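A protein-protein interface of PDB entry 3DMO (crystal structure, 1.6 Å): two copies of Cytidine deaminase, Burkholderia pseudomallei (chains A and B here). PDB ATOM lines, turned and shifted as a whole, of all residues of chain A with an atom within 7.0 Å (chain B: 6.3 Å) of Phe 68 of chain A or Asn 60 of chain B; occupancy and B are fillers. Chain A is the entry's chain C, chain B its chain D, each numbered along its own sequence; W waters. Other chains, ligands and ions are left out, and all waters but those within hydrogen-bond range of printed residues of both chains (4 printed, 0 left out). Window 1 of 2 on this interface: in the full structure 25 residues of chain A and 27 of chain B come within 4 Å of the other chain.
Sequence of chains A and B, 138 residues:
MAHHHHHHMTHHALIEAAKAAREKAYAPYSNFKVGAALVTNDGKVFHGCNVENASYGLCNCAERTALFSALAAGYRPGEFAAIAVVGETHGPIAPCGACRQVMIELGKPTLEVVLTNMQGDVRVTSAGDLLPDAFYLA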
ATOM      1  N   LEU A  38      19.397  20.293  -6.656  1.00  0.00           N
ATOM      2  CA  LEU A  38      18.416  21.071  -5.916  1.00  0.00           C
ATOM      3  C   LEU A  38      18.621  20.835  -4.415  1.00  0.00           C
ATOM      4  O   LEU A  38      18.650  19.674  -3.985  1.00  0.00           O
ATOM      5  CB  LEU A  38      17.014  20.605  -6.328  1.00  0.00           C
ATOM      6  CG  LEU A  38      15.767  21.131  -5.620  1.00  0.00           C
ATOM      7  CD1 LEU A  38      15.498  22.590  -6.012  1.00  0.00           C
ATOM      8  CD2 LEU A  38      14.578  20.249  -5.972  1.00  0.00           C
ATOM      9  N   PHE A  46      18.884  16.882  -4.175  1.00  0.00           N
ATOM     10  CA  PHE A  46      18.340  16.023  -5.218  1.00  0.00           C
ATOM     11  C   PHE A  46      19.051  16.290  -6.535  1.00  0.00           C
ATOM     12  O   PHE A  46      19.129  17.436  -6.984  1.00  0.00           O
ATOM     13  CB  PHE A  46      16.833  16.245  -5.373  1.00  0.00           C
ATOM     14  CG  PHE A  46      16.023  15.736  -4.210  1.00  0.00           C
ATOM     15  CD1 PHE A  46      15.545  14.425  -4.202  1.00  0.00           C
ATOM     16  CD2 PHE A  46      15.736  16.560  -3.130  1.00  0.00           C
ATOM     17  CE1 PHE A  46      14.798  13.943  -3.129  1.00  0.00           C
ATOM     18  CE2 PHE A  46      14.995  16.087  -2.051  1.00  0.00           C
ATOM     19  CZ  PHE A  46      14.520  14.772  -2.057  1.00  0.00           C
ATOM     20  N   LEU A  58       9.124  14.569 -25.790  1.00  0.00           N
ATOM     21  CA  LEU A  58       9.078  13.865 -24.496  1.00  0.00           C
ATOM     22  C   LEU A  58      10.378  13.949 -23.710  1.00  0.00           C
ATOM     23  O   LEU A  58      10.458  13.423 -22.592  1.00  0.00           O
ATOM     24  CB  LEU A  58       8.612  12.403 -24.659  1.00  0.00           C
ATOM     25  CG  LEU A  58       7.197  12.293 -25.244  1.00  0.00           C
ATOM     26  CD1 LEU A  58       6.844  10.867 -25.622  1.00  0.00           C
ATOM     27  CD2 LEU A  58       6.159  12.909 -24.285  1.00  0.00           C
ATOM     28  N   ASN A  60      13.027  15.265 -21.111  1.00  0.00           N
ATOM     29  CA  ASN A  60      12.908  15.993 -19.854  1.00  0.00           C
ATOM     30  C   ASN A  60      14.232  16.641 -19.479  1.00  0.00           C
ATOM     31  O   ASN A  60      15.292  16.052 -19.684  1.00  0.00           O
ATOM     32  CB  ASN A  60      12.437  15.088 -18.711  1.00  0.00           C
ATOM     33  CG  ASN A  60      11.813  15.876 -17.572  1.00  0.00           C
ATOM     34  OD1 ASN A  60      10.874  16.649 -17.778  1.00  0.00           O
ATOM     35  ND2 ASN A  60      12.330  15.688 -16.364  1.00  0.00           N
ATOM     36  N   CYS A  61      14.162  17.850 -18.936  1.00  0.00           N
ATOM     37  CA  CYS A  61      15.355  18.604 -18.562  1.00  0.00           C
ATOM     38  C   CYS A  61      15.835  18.258 -17.156  1.00  0.00           C
ATOM     39  O   CYS A  61      15.048  17.834 -16.316  1.00  0.00           O
ATOM     40  CB  CYS A  61      15.048  20.092 -18.626  1.00  0.00           C
ATOM     41  SG  CYS A  61      14.785  20.709 -20.308  1.00  0.00           S
ATOM     42  N   ALA A  62      17.129  18.467 -16.910  1.00  0.00           N
ATOM     43  CA  ALA A  62      17.730  18.292 -15.575  1.00  0.00           C
ATOM     44  C   ALA A  62      16.993  18.993 -14.435  1.00  0.00           C
ATOM     45  O   ALA A  62      16.763  18.384 -13.379  1.00  0.00           O
ATOM     46  CB  ALA A  62      19.196  18.733 -15.590  1.00  0.00           C
ATOM     47  N   GLU A  63      16.654  20.271 -14.634  1.00  0.00           N
ATOM     48  CA  GLU A  63      15.992  21.078 -13.597  1.00  0.00           C
ATOM     49  C   GLU A  63      14.672  20.431 -13.165  1.00  0.00           C
ATOM     50  O   GLU A  63      14.367  20.325 -11.958  1.00  0.00           O
ATOM     51  CB  GLU A  63      15.738  22.504 -14.106  1.00  0.00           C
ATOM     52  CG  GLU A  63      16.978  23.223 -14.651  1.00  0.00           C
ATOM     53  CD  GLU A  63      17.167  23.044 -16.166  1.00  0.00           C
ATOM     54  OE1 GLU A  63      17.330  21.891 -16.637  1.00  0.00           O
ATOM     55  OE2 GLU A  63      17.163  24.073 -16.890  1.00  0.00           O
ATOM     56  N   ARG A  64      13.908  19.980 -14.160  1.00  0.00           N
ATOM     57  CA  ARG A  64      12.619  19.344 -13.916  1.00  0.00           C
ATOM     58  C   ARG A  64      12.794  17.964 -13.294  1.00  0.00           C
ATOM     59  O   ARG A  64      12.083  17.624 -12.342  1.00  0.00           O
ATOM     60  CB  ARG A  64      11.779  19.304 -15.191  1.00  0.00           C
ATOM     61  CG  ARG A  64      11.176  20.664 -15.517  1.00  0.00           C
ATOM     62  CD  ARG A  64      10.304  20.608 -16.756  1.00  0.00           C
ATOM     63  NE  ARG A  64      11.107  20.617 -17.974  1.00  0.00           N
ATOM     64  CZ  ARG A  64      10.637  20.319 -19.182  1.00  0.00           C
ATOM     65  NH1 ARG A  64       9.362  19.968 -19.332  1.00  0.00           N
ATOM     66  NH2 ARG A  64      11.442  20.352 -20.241  1.00  0.00           N
ATOM     67  N   THR A  65      13.763  17.193 -13.790  1.00  0.00           N
ATOM     68  CA  THR A  65      14.085  15.902 -13.173  1.00  0.00           C
ATOM     69  C   THR A  65      14.352  16.052 -11.678  1.00  0.00           C
ATOM     70  O   THR A  65      13.817  15.279 -10.891  1.00  0.00           O
ATOM     71  CB  THR A  65      15.267  15.195 -13.871  1.00  0.00           C
ATOM     72  OG1 THR A  65      14.908  14.913 -15.226  1.00  0.00           O
ATOM     73  CG2 THR A  65      15.616  13.877 -13.177  1.00  0.00           C
ATOM     74  N   ALA A  66      15.158  17.046 -11.287  1.00  0.00           N
ATOM     75  CA  ALA A  66      15.471  17.264  -9.861  1.00  0.00           C
ATOM     76  C   ALA A  66      14.241  17.628  -9.038  1.00  0.00           C
ATOM     77  O   ALA A  66      14.007  17.051  -7.966  1.00  0.00           O
ATOM     78  CB  ALA A  66      16.554  18.332  -9.703  1.00  0.00           C
ATOM     79  N   LEU A  67      13.460  18.588  -9.543  1.00  0.00           N
ATOM     80  CA  LEU A  67      12.235  19.045  -8.876  1.00  0.00           C
ATOM     81  C   LEU A  67      11.183  17.944  -8.753  1.00  0.00           C
ATOM     82  O   LEU A  67      10.588  17.776  -7.681  1.00  0.00           O
ATOM     83  CB  LEU A  67      11.663  20.288  -9.578  1.00  0.00           C
ATOM     84  CG  LEU A  67      12.440  21.592  -9.322  1.00  0.00           C
ATOM     85  CD1 LEU A  67      12.172  22.604 -10.416  1.00  0.00           C
ATOM     86  CD2 LEU A  67      12.118  22.190  -7.953  1.00  0.00           C
ATOM     87  N   PHE A  68      10.975  17.177  -9.824  1.00  0.00           N
ATOM     88  CA  PHE A  68      10.000  16.080  -9.791  1.00  0.00           C
ATOM     89  C   PHE A  68      10.399  15.021  -8.773  1.00  0.00           C
ATOM     90  O   PHE A  68       9.538  14.495  -8.073  1.00  0.00           O
ATOM     91  CB  PHE A  68       9.796  15.435 -11.171  1.00  0.00           C
ATOM     92  CG  PHE A  68       9.246  16.367 -12.226  1.00  0.00           C
ATOM     93  CD1 PHE A  68       9.528  16.129 -13.573  1.00  0.00           C
ATOM     94  CD2 PHE A  68       8.443  17.469 -11.891  1.00  0.00           C
ATOM     95  CE1 PHE A  68       9.032  16.969 -14.573  1.00  0.00           C
ATOM     96  CE2 PHE A  68       7.941  18.324 -12.887  1.00  0.00           C
ATOM     97  CZ  PHE A  68       8.236  18.071 -14.236  1.00  0.00           C
ATOM     98  N   SER A  69      11.702  14.725  -8.699  1.00  0.00           N
ATOM     99  CA  SER A  69      12.242  13.780  -7.718  1.00  0.00           C
ATOM    100  C   SER A  69      11.985  14.241  -6.290  1.00  0.00           C
ATOM    101  O   SER A  69      11.602  13.445  -5.428  1.00  0.00           O
ATOM    102  CB  SER A  69      13.745  13.586  -7.921  1.00  0.00           C
ATOM    103  OG  SER A  69      14.008  12.835  -9.087  1.00  0.00           O
ATOM    104  N   ALA A  70      12.201  15.529  -6.038  1.00  0.00           N
ATOM    105  CA  ALA A  70      11.981  16.103  -4.710  1.00  0.00           C
ATOM    106  C   ALA A  70      10.499  16.046  -4.304  1.00  0.00           C
ATOM    107  O   ALA A  70      10.169  15.707  -3.160  1.00  0.00           O
ATOM    108  CB  ALA A  70      12.497  17.520  -4.665  1.00  0.00           C
ATOM    109  N   LEU A  71       9.609  16.379  -5.235  1.00  0.00           N
ATOM    110  CA  LEU A  71       8.162  16.242  -5.015  1.00  0.00           C
ATOM    111  C   LEU A  71       7.783  14.795  -4.704  1.00  0.00           C
ATOM    112  O   LEU A  71       7.010  14.534  -3.777  1.00  0.00           O
ATOM    113  CB  LEU A  71       7.374  16.751  -6.237  1.00  0.00           C
ATOM    114  CG  LEU A  71       6.932  18.217  -6.291  1.00  0.00           C
ATOM    115  CD1 LEU A  71       5.707  18.432  -5.405  1.00  0.00           C
ATOM    116  CD2 LEU A  71       8.060  19.201  -5.919  1.00  0.00           C
ATOM    117  N   ALA A  72       8.357  13.860  -5.461  1.00  0.00           N
ATOM    118  CA  ALA A  72       8.093  12.434  -5.288  1.00  0.00           C
ATOM    119  C   ALA A  72       8.561  11.944  -3.918  1.00  0.00           C
ATOM    120  O   ALA A  72       8.025  10.974  -3.392  1.00  0.00           O
ATOM    121  CB  ALA A  72       8.741  11.631  -6.395  1.00  0.00           C
ATOM    122  N   ALA A  73       9.557  12.623  -3.348  1.00  0.00           N
ATOM    123  CA  ALA A  73      10.062  12.275  -2.019  1.00  0.00           C
ATOM    124  C   ALA A  73       9.186  12.834  -0.907  1.00  0.00           C
ATOM    125  O   ALA A  73       9.347  12.459   0.257  1.00  0.00           O
ATOM    126  CB  ALA A  73      11.504  12.746  -1.848  1.00  0.00           C
ATOM    127  N   GLY A  74       8.277  13.740  -1.255  1.00  0.00           N
ATOM    128  CA  GLY A  74       7.352  14.312  -0.285  1.00  0.00           C
ATOM    129  C   GLY A  74       7.530  15.794  -0.014  1.00  0.00           C
ATOM    130  O   GLY A  74       6.770  16.377   0.763  1.00  0.00           O
ATOM    131  N   VAL A 102       8.139  25.550 -14.532  1.00  0.00           N
ATOM    132  CA  VAL A 102       8.092  24.561 -13.456  1.00  0.00           C
ATOM    133  C   VAL A 102       8.822  25.078 -12.215  1.00  0.00           C
ATOM    134  O   VAL A 102       8.336  24.911 -11.096  1.00  0.00           O
ATOM    135  CB  VAL A 102       8.614  23.179 -13.924  1.00  0.00           C
ATOM    136  CG1 VAL A 102       8.790  22.214 -12.741  1.00  0.00           C
ATOM    137  CG2 VAL A 102       7.643  22.590 -14.945  1.00  0.00           C
ATOM    138  N   LEU A 106       7.015  25.332  -8.473  1.00  0.00           N
ATOM    139  CA  LEU A 106       7.516  24.449  -7.421  1.00  0.00           C
ATOM    140  C   LEU A 106       8.531  25.120  -6.501  1.00  0.00           C
ATOM    141  O   LEU A 106       8.616  24.783  -5.318  1.00  0.00           O
ATOM    142  CB  LEU A 106       8.091  23.162  -8.017  1.00  0.00           C
ATOM    143  CG  LEU A 106       7.175  22.344  -8.947  1.00  0.00           C
ATOM    144  CD1 LEU A 106       7.876  21.065  -9.385  1.00  0.00           C
ATOM    145  CD2 LEU A 106       5.802  22.050  -8.330  1.00  0.00           C
ATOM    146  N   CYS B  49       5.200  10.182  -8.749  1.00  0.00           N
ATOM    147  CA  CYS B  49       3.842  10.680  -8.654  1.00  0.00           C
ATOM    148  C   CYS B  49       3.640  11.732  -9.734  1.00  0.00           C
ATOM    149  O   CYS B  49       4.619  12.226 -10.320  1.00  0.00           O
ATOM    150  CB  CYS B  49       3.584  11.240  -7.247  1.00  0.00           C
ATOM    151  SG  CYS B  49       4.674  12.602  -6.800  1.00  0.00           S
ATOM    152  N   ASN B  50       2.388  12.059 -10.037  1.00  0.00           N
ATOM    153  CA  ASN B  50       2.149  13.172 -10.944  1.00  0.00           C
ATOM    154  C   ASN B  50       2.481  14.502 -10.268  1.00  0.00           C
ATOM    155  O   ASN B  50       2.363  14.640  -9.046  1.00  0.00           O
ATOM    156  CB  ASN B  50       0.752  13.133 -11.600  1.00  0.00           C
ATOM    157  CG  ASN B  50      -0.387  13.037 -10.603  1.00  0.00           C
ATOM    158  OD1 ASN B  50      -0.269  12.399  -9.553  1.00  0.00           O
ATOM    159  ND2 ASN B  50      -1.523  13.650 -10.950  1.00  0.00           N
ATOM    160  N   VAL B  51       2.988  15.440 -11.055  1.00  0.00           N
ATOM    161  CA  VAL B  51       3.364  16.760 -10.567  1.00  0.00           C
ATOM    162  C   VAL B  51       2.812  17.746 -11.568  1.00  0.00           C
ATOM    163  O   VAL B  51       3.308  17.847 -12.694  1.00  0.00           O
ATOM    164  CB  VAL B  51       4.905  16.938 -10.450  1.00  0.00           C
ATOM    165  CG1 VAL B  51       5.250  18.314  -9.889  1.00  0.00           C
ATOM    166  CG2 VAL B  51       5.517  15.822  -9.599  1.00  0.00           C
ATOM    167  N   GLU B  52       1.785  18.468 -11.139  1.00  0.00           N
ATOM    168  CA  GLU B  52       1.041  19.350 -12.018  1.00  0.00           C
ATOM    169  C   GLU B  52       1.597  20.774 -12.046  1.00  0.00           C
ATOM    170  O   GLU B  52       2.455  21.141 -11.242  1.00  0.00           O
ATOM    171  CB  GLU B  52      -0.449  19.321 -11.650  1.00  0.00           C
ATOM    172  CG  GLU B  52      -1.029  17.939 -11.892  1.00  0.00           C
ATOM    173  CD  GLU B  52      -2.539  17.837 -11.785  1.00  0.00           C
ATOM    174  OE1 GLU B  52      -3.080  16.839 -12.315  1.00  0.00           O
ATOM    175  OE2 GLU B  52      -3.180  18.718 -11.170  1.00  0.00           O
ATOM    176  N   ASN B  53       1.126  21.550 -13.022  1.00  0.00           N
ATOM    177  CA  ASN B  53       1.522  22.946 -13.190  1.00  0.00           C
ATOM    178  C   ASN B  53       0.294  23.721 -13.644  1.00  0.00           C
ATOM    179  O   ASN B  53      -0.603  23.131 -14.242  1.00  0.00           O
ATOM    180  CB  ASN B  53       2.644  23.046 -14.230  1.00  0.00           C
ATOM    181  CG  ASN B  53       3.314  24.408 -14.242  1.00  0.00           C
ATOM    182  OD1 ASN B  53       2.853  25.336 -14.922  1.00  0.00           O
ATOM    183  ND2 ASN B  53       4.422  24.533 -13.512  1.00  0.00           N
ATOM    184  N   TYR B  56      -1.061  23.554 -17.924  1.00  0.00           N
ATOM    185  CA  TYR B  56      -1.283  22.102 -17.940  1.00  0.00           C
ATOM    186  C   TYR B  56      -0.253  21.321 -18.750  1.00  0.00           C
ATOM    187  O   TYR B  56       0.113  20.206 -18.391  1.00  0.00           O
ATOM    188  CB  TYR B  56      -2.692  21.779 -18.444  1.00  0.00           C
ATOM    189  CG  TYR B  56      -3.818  22.062 -17.475  1.00  0.00           C
ATOM    190  CD1 TYR B  56      -5.105  21.605 -17.748  1.00  0.00           C
ATOM    191  CD2 TYR B  56      -3.610  22.783 -16.287  1.00  0.00           C
ATOM    192  CE1 TYR B  56      -6.159  21.858 -16.883  1.00  0.00           C
ATOM    193  CE2 TYR B  56      -4.665  23.040 -15.405  1.00  0.00           C
ATOM    194  CZ  TYR B  56      -5.936  22.569 -15.714  1.00  0.00           C
ATOM    195  OH  TYR B  56      -7.003  22.801 -14.874  1.00  0.00           O
ATOM    196  N   LEU B  58       2.725  21.437 -18.834  1.00  0.00           N
ATOM    197  CA  LEU B  58       3.951  21.213 -18.068  1.00  0.00           C
ATOM    198  C   LEU B  58       3.779  20.128 -16.999  1.00  0.00           C
ATOM    199  O   LEU B  58       4.717  19.814 -16.282  1.00  0.00           O
ATOM    200  CB  LEU B  58       4.423  22.529 -17.423  1.00  0.00           C
ATOM    201  CG  LEU B  58       5.111  23.639 -18.241  1.00  0.00           C
ATOM    202  CD1 LEU B  58       6.496  23.199 -18.682  1.00  0.00           C
ATOM    203  CD2 LEU B  58       4.301  24.135 -19.431  1.00  0.00           C
ATOM    204  N   CYS B  59       2.572  19.572 -16.900  1.00  0.00           N
ATOM    205  CA  CYS B  59       2.315  18.467 -15.964  1.00  0.00           C
ATOM    206  C   CYS B  59       3.190  17.262 -16.307  1.00  0.00           C
ATOM    207  O   CYS B  59       3.453  16.991 -17.483  1.00  0.00           O
ATOM    208  CB  CYS B  59       0.841  18.056 -15.997  1.00  0.00           C
ATOM    209  SG  CYS B  59      -0.288  19.302 -15.287  1.00  0.00           S
ATOM    210  N   ASN B  60       3.649  16.560 -15.277  1.00  0.00           N
ATOM    211  CA  ASN B  60       4.387  15.316 -15.461  1.00  0.00           C
ATOM    212  C   ASN B  60       3.683  14.157 -14.772  1.00  0.00           C
ATOM    213  O   ASN B  60       3.176  14.310 -13.658  1.00  0.00           O
ATOM    214  CB  ASN B  60       5.813  15.424 -14.920  1.00  0.00           C
ATOM    215  CG  ASN B  60       6.731  14.365 -15.508  1.00  0.00           C
ATOM    216  OD1 ASN B  60       6.867  14.265 -16.733  1.00  0.00           O
ATOM    217  ND2 ASN B  60       7.353  13.566 -14.649  1.00  0.00           N
ATOM    218  N   CYS B  61       3.666  13.008 -15.445  1.00  0.00           N
ATOM    219  CA  CYS B  61       3.018  11.798 -14.937  1.00  0.00           C
ATOM    220  C   CYS B  61       3.876  11.012 -13.961  1.00  0.00           C
ATOM    221  O   CYS B  61       5.105  11.082 -14.002  1.00  0.00           O
ATOM    222  CB  CYS B  61       2.676  10.887 -16.100  1.00  0.00           C
ATOM    223  SG  CYS B  61       1.400  11.517 -17.191  1.00  0.00           S
ATOM    224  N   ALA B  62       3.209  10.245 -13.094  1.00  0.00           N
ATOM    225  CA  ALA B  62       3.876   9.392 -12.118  1.00  0.00           C
ATOM    226  C   ALA B  62       4.905   8.418 -12.710  1.00  0.00           C
ATOM    227  O   ALA B  62       6.011   8.274 -12.189  1.00  0.00           O
ATOM    228  CB  ALA B  62       2.827   8.631 -11.301  1.00  0.00           C
ATOM    229  N   GLU B  63       4.542   7.757 -13.808  1.00  0.00           N
ATOM    230  CA  GLU B  63       5.413   6.783 -14.437  1.00  0.00           C
ATOM    231  C   GLU B  63       6.716   7.471 -14.850  1.00  0.00           C
ATOM    232  O   GLU B  63       7.816   6.956 -14.604  1.00  0.00           O
ATOM    233  CB  GLU B  63       4.737   6.174 -15.671  1.00  0.00           C
ATOM    234  CG  GLU B  63       3.394   5.478 -15.402  1.00  0.00           C
ATOM    235  CD  GLU B  63       2.177   6.386 -15.595  1.00  0.00           C
ATOM    236  OE1 GLU B  63       2.086   7.442 -14.943  1.00  0.00           O
ATOM    237  OE2 GLU B  63       1.296   6.030 -16.410  1.00  0.00           O
ATOM    238  N   ARG B  64       6.583   8.638 -15.481  1.00  0.00           N
ATOM    239  CA  ARG B  64       7.755   9.377 -15.940  1.00  0.00           C
ATOM    240  C   ARG B  64       8.588   9.946 -14.803  1.00  0.00           C
ATOM    241  O   ARG B  64       9.812   9.903 -14.874  1.00  0.00           O
ATOM    242  CB  ARG B  64       7.378  10.446 -16.962  1.00  0.00           C
ATOM    243  CG  ARG B  64       7.007   9.833 -18.309  1.00  0.00           C
ATOM    244  CD  ARG B  64       6.638  10.900 -19.302  1.00  0.00           C
ATOM    245  NE  ARG B  64       5.275  11.369 -19.077  1.00  0.00           N
ATOM    246  CZ  ARG B  64       4.777  12.502 -19.560  1.00  0.00           C
ATOM    247  NH1 ARG B  64       5.524  13.301 -20.326  1.00  0.00           N
ATOM    248  NH2 ARG B  64       3.524  12.837 -19.286  1.00  0.00           N
ATOM    249  N   THR B  65       7.928  10.430 -13.747  1.00  0.00           N
ATOM    250  CA  THR B  65       8.610  10.882 -12.526  1.00  0.00           C
ATOM    251  C   THR B  65       9.490   9.771 -11.937  1.00  0.00           C
ATOM    252  O   THR B  65      10.664  10.002 -11.641  1.00  0.00           O
ATOM    253  CB  THR B  65       7.611  11.382 -11.457  1.00  0.00           C
ATOM    254  OG1 THR B  65       6.942  12.557 -11.934  1.00  0.00           O
ATOM    255  CG2 THR B  65       8.327  11.732 -10.153  1.00  0.00           C
ATOM    256  N   ALA B  66       8.931   8.567 -11.800  1.00  0.00           N
ATOM    257  CA  ALA B  66       9.691   7.414 -11.294  1.00  0.00           C
ATOM    258  C   ALA B  66      10.913   7.084 -12.152  1.00  0.00           C
ATOM    259  O   ALA B  66      12.019   6.907 -11.627  1.00  0.00           O
ATOM    260  CB  ALA B  66       8.794   6.193 -11.163  1.00  0.00           C
ATOM    261  N   PHE B  68      12.482   9.044 -14.468  1.00  0.00           N
ATOM    262  CA  PHE B  68      13.451  10.156 -14.480  1.00  0.00           C
ATOM    263  C   PHE B  68      14.296  10.175 -13.200  1.00  0.00           C
ATOM    264  O   PHE B  68      15.508  10.444 -13.245  1.00  0.00           O
ATOM    265  CB  PHE B  68      12.762  11.518 -14.707  1.00  0.00           C
ATOM    266  CG  PHE B  68      12.028  11.631 -16.028  1.00  0.00           C
ATOM    267  CD1 PHE B  68      10.973  12.534 -16.160  1.00  0.00           C
ATOM    268  CD2 PHE B  68      12.377  10.833 -17.120  1.00  0.00           C
ATOM    269  CE1 PHE B  68      10.273  12.650 -17.365  1.00  0.00           C
ATOM    270  CE2 PHE B  68      11.682  10.934 -18.334  1.00  0.00           C
ATOM    271  CZ  PHE B  68      10.628  11.854 -18.448  1.00  0.00           C
ATOM    272  N   SER B  69      13.649   9.852 -12.073  1.00  0.00           N
ATOM    273  CA  SER B  69      14.320   9.760 -10.778  1.00  0.00           C
ATOM    274  C   SER B  69      15.373   8.654 -10.781  1.00  0.00           C
ATOM    275  O   SER B  69      16.496   8.846 -10.311  1.00  0.00           O
ATOM    276  CB  SER B  69      13.299   9.501  -9.673  1.00  0.00           C
ATOM    277  OG  SER B  69      12.611  10.687  -9.331  1.00  0.00           O
HETATM  278  O   HOH W   1      11.965  12.914 -11.722  1.00  0.00           O
HETATM  279  O   HOH W   2       8.376  13.438 -20.752  1.00  0.00           O
HETATM  280  O   HOH W   3       6.022   9.680  -5.120  1.00  0.00           O
HETATM  281  O   HOH W   4       7.223  19.211 -17.499  1.00  0.00           O
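The side-chain hydroxyl (OG) of Ser 69 of chain B is in hydrogen-bond range of the side-chain hydroxyl (OG) of Ser 69 of chain A (2.6 Å).
Water W2 bridges O of Leu 58 of chain A (2.8 Å) and NH1 of Arg 64 of chain B (2.9 Å). Water W4 lies within hydrogen-bond range of O of Leu 58 of chain B and NH1 of Arg 64 of chain A. Water W3 lies within hydrogen-bond range of the backbone carbonyl oxygen of Ala 72 of chain A (2.9 Å) and the side-chain sulfur of Cys 49 of chain B (3.6 Å). Water W1 lies within hydrogen-bond range of the backbone carbonyl oxygen of Thr 65 of chain A, the backbone carbonyl oxygen of Thr 65 of chain B, the side-chain hydroxyl of Ser 69 of chain B and the side-chain hydroxyl of Ser 69 of chain A.
Among the printed residues, merely in contact across the chains: Thr 65 of chain A with Phe 68 of chain B, Asn 60 of chain A with Phe 68 of chain B, Phe 68 of chain A with Asn 60 of chain B, Phe 68 of chain A with Thr 65 of chain B, Val 102 of chain A with Asn 53 of chain B, Ala 72 of chain A with Cys 49 of chain B, Ala 72 of chain A with Thr 65 of chain B, Leu 106 of chain A with Val 51 of chain B, Phe 68 of chain A with Val 51 of chain B, Leu 71 of chain A with Val 51 of chain B and Val 102 of chain A with Leu 58 of chain B.
Of the 17 printed residues of chain B, 8 touch a printed residue of chain A. Of the 20 printed residues of chain A, 8 touch a printed residue of chain B. Hydrophobic or aromatic side chains of chain A that line the printed part of chain B: Phe 68, Leu 71, Ala 72, Val 102 and Leu 106. Along chain A the printed residues that touch a printed residue of chain B span positions 60 to 106. Among the printed residues, 12 pairs touch across the chains.
Asn 60 of chain B touches just one residue of chain A: Phe 68. Of the printed residues of chain A, Thr 65 of chain B touches Phe 68 and Ala 72. Printed residues of chain B within 4 Å of Thr 65 of chain A: Phe 68 (3.4 Å). Of the printed residues of chain A, Asn 53 of chain B touches Val 102 (3.7 Å). Of the printed residues of chain A, Leu 58 of chain B touches Val 102 (3.96 Å). Ala 70 of chain A touches none of the printed residues of chain B. Glu 52 of chain B touches none of the printed residues of chain A. The nearest printed residue of chain B that does not touch Phe 68 of chain A is Leu 58 of chain B (4.4 Å). The nearest residue of chain A that does not touch Asn 60 of chain B is Asn 60 of chain A (4.8 Å).
Asn 60 of chain A touches Phe 68 of chain B, and with the chains exchanged Phe 68 of chain A touches Asn 60 of chain B. Thr 65 of chain A touches Phe 68 of chain B, and with the chains exchanged Phe 68 of chain A touches Thr 65 of chain B. Ser 69 of chain A touches its own counterpart, Ser 69 of chain B. Positions printed for both chains: 58, 60, 61, 62, 63, 64, 65, 66, 68 and 69. Of the 12 pairs that touch across the chains among the printed residues, 5 have their exchanged pair printed and touching as well.
The backbone carbonyl oxygen of Cys 61 of chain B lies within hydrogen-bond range of the side-chain hydroxyl of Thr 65 of chain B (3.1 Å). N of Asn 53 of chain B sits at hydrogen-bond distance from SG of Cys 59 of chain B (3.5 Å). OG of Ser 69 of chain A lies within hydrogen-bond range of O of Thr 65 of chain A (3.0 Å). The backbone carbonyl oxygen (O) of Cys 61 of chain A is in hydrogen-bond range of the side-chain hydroxyl (OG1) of Thr 65 of chain A (3.1 Å). The backbone carbonyl oxygen (O) of Cys 49 of chain B lies within hydrogen-bond range of the side-chain hydroxyl (OG1) of Thr 65 of chain B, 2.8 Å away. The backbone NH of Val 51 of chain B lies within hydrogen-bond range of the backbone carbonyl oxygen of Asn 60 of chain B, 2.8 Å away.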
